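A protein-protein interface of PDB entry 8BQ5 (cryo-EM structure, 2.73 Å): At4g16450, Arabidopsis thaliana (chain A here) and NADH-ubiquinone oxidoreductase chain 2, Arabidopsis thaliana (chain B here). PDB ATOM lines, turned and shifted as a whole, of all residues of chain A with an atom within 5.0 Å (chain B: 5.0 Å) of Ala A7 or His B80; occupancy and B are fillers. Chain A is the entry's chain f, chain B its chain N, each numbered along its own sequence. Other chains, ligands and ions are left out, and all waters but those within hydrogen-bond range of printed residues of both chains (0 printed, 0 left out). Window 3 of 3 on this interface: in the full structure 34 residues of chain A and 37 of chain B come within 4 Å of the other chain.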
ATOM      1  N   ASP A   4      -3.961  24.409  10.113  1.00  0.00           N
ATOM      2  CA  ASP A   4      -5.103  23.559  10.540  1.00  0.00           C
ATOM      3  C   ASP A   4      -6.198  23.625   9.472  1.00  0.00           C
ATOM      4  O   ASP A   4      -6.816  24.694   9.371  1.00  0.00           O
ATOM      5  CB  ASP A   4      -5.642  24.004  11.899  1.00  0.00           C
ATOM      6  CG  ASP A   4      -6.449  22.938  12.621  1.00  0.00           C
ATOM      7  OD1 ASP A   4      -6.660  21.855  12.040  1.00  0.00           O
ATOM      8  OD2 ASP A   4      -6.851  23.197  13.766  1.00  0.00           O
ATOM      9  N   ILE A   5      -6.451  22.524   8.755  1.00  0.00           N
ATOM     10  CA  ILE A   5      -7.470  22.479   7.657  1.00  0.00           C
ATOM     11  C   ILE A   5      -8.894  22.408   8.224  1.00  0.00           C
ATOM     12  O   ILE A   5      -9.830  22.693   7.461  1.00  0.00           O
ATOM     13  CB  ILE A   5      -7.165  21.303   6.701  1.00  0.00           C
ATOM     14  CG1 ILE A   5      -7.779  21.488   5.308  1.00  0.00           C
ATOM     15  CG2 ILE A   5      -7.565  19.968   7.312  1.00  0.00           C
ATOM     16  CD1 ILE A   5      -7.340  22.742   4.600  1.00  0.00           C
ATOM     17  N   THR A   6      -9.056  22.062   9.504  1.00  0.00           N
ATOM     18  CA  THR A   6     -10.397  21.917  10.133  1.00  0.00           C
ATOM     19  C   THR A   6     -11.360  22.994   9.627  1.00  0.00           C
ATOM     20  O   THR A   6     -11.068  24.181   9.829  1.00  0.00           O
ATOM     21  CB  THR A   6     -10.294  21.925  11.663  1.00  0.00           C
ATOM     22  OG1 THR A   6      -9.391  20.895  12.061  1.00  0.00           O
ATOM     23  CG2 THR A   6     -11.630  21.723  12.345  1.00  0.00           C
ATOM     24  N   ALA A   7     -12.449  22.591   8.970  1.00  0.00           N
ATOM     25  CA  ALA A   7     -13.456  23.509   8.463  1.00  0.00           C
ATOM     26  C   ALA A   7     -14.546  23.743   9.502  1.00  0.00           C
ATOM     27  O   ALA A   7     -14.758  22.941  10.413  1.00  0.00           O
ATOM     28  CB  ALA A   7     -14.070  22.977   7.168  1.00  0.00           C
ATOM     29  N   LEU A   8     -15.236  24.875   9.354  1.00  0.00           N
ATOM     30  CA  LEU A   8     -16.302  25.221  10.288  1.00  0.00           C
ATOM     31  C   LEU A   8     -17.475  24.255  10.170  1.00  0.00           C
ATOM     32  O   LEU A   8     -17.959  23.727  11.178  1.00  0.00           O
ATOM     33  CB  LEU A   8     -16.760  26.658  10.046  1.00  0.00           C
ATOM     34  CG  LEU A   8     -17.965  27.109  10.869  1.00  0.00           C
ATOM     35  CD1 LEU A   8     -17.556  27.337  12.314  1.00  0.00           C
ATOM     36  CD2 LEU A   8     -18.581  28.363  10.270  1.00  0.00           C
ATOM     37  N   GLU A   9     -17.942  24.009   8.951  1.00  0.00           N
ATOM     38  CA  GLU A   9     -19.041  23.085   8.706  1.00  0.00           C
ATOM     39  C   GLU A   9     -18.460  21.742   8.286  1.00  0.00           C
ATOM     40  O   GLU A   9     -17.657  21.672   7.350  1.00  0.00           O
ATOM     41  CB  GLU A   9     -19.993  23.629   7.640  1.00  0.00           C
ATOM     42  CG  GLU A   9     -19.305  24.290   6.457  1.00  0.00           C
ATOM     43  CD  GLU A   9     -20.211  24.410   5.248  1.00  0.00           C
ATOM     44  OE1 GLU A   9     -20.693  23.367   4.758  1.00  0.00           O
ATOM     45  OE2 GLU A   9     -20.441  25.547   4.785  1.00  0.00           O
ATOM     46  N   LYS A  10     -18.864  20.684   8.983  1.00  0.00           N
ATOM     47  CA  LYS A  10     -18.298  19.366   8.754  1.00  0.00           C
ATOM     48  C   LYS A  10     -18.720  18.822   7.392  1.00  0.00           C
ATOM     49  O   LYS A  10     -19.787  19.143   6.863  1.00  0.00           O
ATOM     50  CB  LYS A  10     -18.729  18.406   9.863  1.00  0.00           C
ATOM     51  CG  LYS A  10     -18.089  18.679  11.218  1.00  0.00           C
ATOM     52  CD  LYS A  10     -16.668  19.212  11.088  1.00  0.00           C
ATOM     53  CE  LYS A  10     -15.969  19.250  12.441  1.00  0.00           C
ATOM     54  NZ  LYS A  10     -14.523  18.893  12.349  1.00  0.00           N
ATOM     55  N   PHE A  88     -16.512  17.205   0.992  1.00  0.00           N
ATOM     56  CA  PHE A  88     -17.434  18.335   0.991  1.00  0.00           C
ATOM     57  C   PHE A  88     -18.441  18.251  -0.147  1.00  0.00           C
ATOM     58  O   PHE A  88     -19.529  18.830  -0.049  1.00  0.00           O
ATOM     59  CB  PHE A  88     -16.653  19.645   0.906  1.00  0.00           C
ATOM     60  CG  PHE A  88     -15.886  19.966   2.148  1.00  0.00           C
ATOM     61  CD1 PHE A  88     -16.538  20.410   3.285  1.00  0.00           C
ATOM     62  CD2 PHE A  88     -14.514  19.800   2.189  1.00  0.00           C
ATOM     63  CE1 PHE A  88     -15.832  20.699   4.433  1.00  0.00           C
ATOM     64  CE2 PHE A  88     -13.805  20.085   3.335  1.00  0.00           C
ATOM     65  CZ  PHE A  88     -14.465  20.536   4.458  1.00  0.00           C
ATOM     66  N   THR B  77     -15.321  28.089   4.167  1.00  0.00           N
ATOM     67  CA  THR B  77     -15.159  27.996   5.612  1.00  0.00           C
ATOM     68  C   THR B  77     -14.031  27.062   6.018  1.00  0.00           C
ATOM     69  O   THR B  77     -13.882  26.772   7.208  1.00  0.00           O
ATOM     70  CB  THR B  77     -16.459  27.526   6.266  1.00  0.00           C
ATOM     71  OG1 THR B  77     -16.825  26.249   5.733  1.00  0.00           O
ATOM     72  CG2 THR B  77     -17.575  28.523   6.005  1.00  0.00           C
ATOM     73  N   ILE B  78     -13.247  26.573   5.060  1.00  0.00           N
ATOM     74  CA  ILE B  78     -12.176  25.641   5.375  1.00  0.00           C
ATOM     75  C   ILE B  78     -11.034  26.377   6.068  1.00  0.00           C
ATOM     76  O   ILE B  78     -10.806  27.575   5.848  1.00  0.00           O
ATOM     77  CB  ILE B  78     -11.701  24.927   4.097  1.00  0.00           C
ATOM     78  CG1 ILE B  78     -11.330  23.480   4.400  1.00  0.00           C
ATOM     79  CG2 ILE B  78     -10.528  25.654   3.456  1.00  0.00           C
ATOM     80  CD1 ILE B  78     -11.452  22.585   3.204  1.00  0.00           C
ATOM     81  N   ALA B  79     -10.320  25.650   6.930  1.00  0.00           N
ATOM     82  CA  ALA B  79      -9.196  26.189   7.697  1.00  0.00           C
ATOM     83  C   ALA B  79      -9.589  27.450   8.465  1.00  0.00           C
ATOM     84  O   ALA B  79      -8.838  28.425   8.513  1.00  0.00           O
ATOM     85  CB  ALA B  79      -7.989  26.458   6.794  1.00  0.00           C
ATOM     86  N   HIS B  80     -10.773  27.427   9.081  1.00  0.00           N
ATOM     87  CA  HIS B  80     -11.289  28.637   9.717  1.00  0.00           C
ATOM     88  C   HIS B  80     -10.451  29.057  10.920  1.00  0.00           C
ATOM     89  O   HIS B  80     -10.337  30.254  11.197  1.00  0.00           O
ATOM     90  CB  HIS B  80     -12.757  28.450  10.111  1.00  0.00           C
ATOM     91  CG  HIS B  80     -12.970  27.545  11.284  1.00  0.00           C
ATOM     92  ND1 HIS B  80     -12.500  26.250  11.322  1.00  0.00           N
ATOM     93  CD2 HIS B  80     -13.613  27.746  12.459  1.00  0.00           C
ATOM     94  CE1 HIS B  80     -12.842  25.693  12.470  1.00  0.00           C
ATOM     95  NE2 HIS B  80     -13.517  26.580  13.178  1.00  0.00           N
ATOM     96  N   LEU B  81      -9.863  28.103  11.646  1.00  0.00           N
ATOM     97  CA  LEU B  81      -8.975  28.469  12.746  1.00  0.00           C
ATOM     98  C   LEU B  81      -7.727  29.180  12.239  1.00  0.00           C
ATOM     99  O   LEU B  81      -7.282  30.167  12.837  1.00  0.00           O
ATOM    100  CB  LEU B  81      -8.588  27.230  13.552  1.00  0.00           C
ATOM    101  CG  LEU B  81      -9.718  26.527  14.302  1.00  0.00           C
ATOM    102  CD1 LEU B  81      -9.172  25.356  15.101  1.00  0.00           C
ATOM    103  CD2 LEU B  81     -10.448  27.503  15.204  1.00  0.00           C
ATOM    104  N   PHE B  82      -7.145  28.687  11.145  1.00  0.00           N
ATOM    105  CA  PHE B  82      -5.940  29.297  10.593  1.00  0.00           C
ATOM    106  C   PHE B  82      -6.210  30.704  10.073  1.00  0.00           C
ATOM    107  O   PHE B  82      -5.379  31.604  10.236  1.00  0.00           O
ATOM    108  CB  PHE B  82      -5.375  28.408   9.487  1.00  0.00           C
ATOM    109  CG  PHE B  82      -4.248  29.032   8.723  1.00  0.00           C
ATOM    110  CD1 PHE B  82      -2.945  28.914   9.167  1.00  0.00           C
ATOM    111  CD2 PHE B  82      -4.490  29.717   7.543  1.00  0.00           C
ATOM    112  CE1 PHE B  82      -1.906  29.482   8.461  1.00  0.00           C
ATOM    113  CE2 PHE B  82      -3.457  30.285   6.832  1.00  0.00           C
ATOM    114  CZ  PHE B  82      -2.161  30.167   7.292  1.00  0.00           C
ATOM    115  N   TRP B  83      -7.355  30.908   9.430  1.00  0.00           N
ATOM    116  CA  TRP B  83      -7.720  32.198   8.861  1.00  0.00           C
ATOM    117  C   TRP B  83      -8.473  33.088   9.842  1.00  0.00           C
ATOM    118  O   TRP B  83      -8.881  34.189   9.464  1.00  0.00           O
ATOM    119  CB  TRP B  83      -8.580  31.994   7.609  1.00  0.00           C
ATOM    120  CG  TRP B  83      -7.851  31.395   6.450  1.00  0.00           C
ATOM    121  CD1 TRP B  83      -8.042  30.156   5.920  1.00  0.00           C
ATOM    122  CD2 TRP B  83      -6.841  32.022   5.649  1.00  0.00           C
ATOM    123  NE1 TRP B  83      -7.200  29.960   4.854  1.00  0.00           N
ATOM    124  CE2 TRP B  83      -6.454  31.093   4.664  1.00  0.00           C
ATOM    125  CE3 TRP B  83      -6.221  33.274   5.676  1.00  0.00           C
ATOM    126  CZ2 TRP B  83      -5.477  31.377   3.714  1.00  0.00           C
ATOM    127  CZ3 TRP B  83      -5.252  33.553   4.733  1.00  0.00           C
ATOM    128  CH2 TRP B  83      -4.889  32.609   3.765  1.00  0.00           C
ATOM    129  N   ASN B  84      -8.653  32.641  11.086  1.00  0.00           N
ATOM    130  CA  ASN B  84      -9.592  33.298  11.990  1.00  0.00           C
ATOM    131  C   ASN B  84      -9.193  34.736  12.290  1.00  0.00           C
ATOM    132  O   ASN B  84     -10.053  35.619  12.383  1.00  0.00           O
ATOM    133  CB  ASN B  84      -9.709  32.512  13.289  1.00  0.00           C
ATOM    134  CG  ASN B  84     -10.674  33.149  14.256  1.00  0.00           C
ATOM    135  OD1 ASN B  84     -11.867  33.247  13.980  1.00  0.00           O
ATOM    136  ND2 ASN B  84     -10.161  33.598  15.395  1.00  0.00           N
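OG1 of Thr A6 is in hydrogen-bond range of OD1 of Asp A4 (2.9 Å).
Of the printed residues of chain B, Asp A4 touches Ala B79 (3.3 Å), Leu B81 (3.4 Å) and Phe B82 (3.99 Å).
Printed residues of chain B within 4 Å of Ile A5: Ile B78 and Ala B79.
Ala A7 touches three residues of chain B.
Of the printed residues of chain B, Leu A8 touches Thr B77 (3.2 Å) and His B80 (3.6 Å).
Printed residues of chain A within 4 Å of Ile B78: Ile A5, Ala A7 and Phe A88.
Of chain A, only Thr A6 (2.9 Å), Ala A7 (3.7 Å) and Leu A8 (3.6 Å) come within 4 Å of His B80.
Of the printed residues of chain A, Leu B81 touches Asp A4 (3.4 Å).
The nearest residue of chain A that does not touch His B80 is Asp A4 (4.8 Å).
Of the 8 printed residues of chain B, 6 touch a printed residue of chain A.
Hydrophobic or aromatic side chains of chain A that line the printed part of chain B: Ala A7, Leu A8 and Phe A88.
Among the printed residues, no Asp or Glu carboxylate lies within 4 Å of a Lys or Arg side-chain nitrogen of the other chain.
ND1 of His B80 sits at hydrogen-bond distance from O of Thr A6 (2.9 Å).
N of Leu A8 is in hydrogen-bond range of O of Thr B77 (3.2 Å).
O of Ile A5 is in hydrogen-bond range of N of Ala B79 (3.0 Å).
The backbone carbonyl oxygen of Thr A6 lies within hydrogen-bond range of the backbone NH of Ala B79, at 3.3 Å.
CA of Ala B79 touches O of Asp A4, 3.3 Å away.
Asp A4 touches Leu B81 (OD2 to CD1, 3.4 Å).
Asp A4 touches Phe B82.
Ile B78 touches Ile A5 (CG1 to O, 3.5 Å).
Thr B77 touches Ala A7.
CB of Ala A7 touches CA of Ile B78, 3.7 Å away.
Ala A7 touches His B80 (C to ND1, 3.7 Å).
N of Leu A8 touches ND1 of His B80, 3.6 Å away.
CG of Glu A9 touches OG1 of Thr B77, at 3.2 Å.
Ile B78 touches Phe A88.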
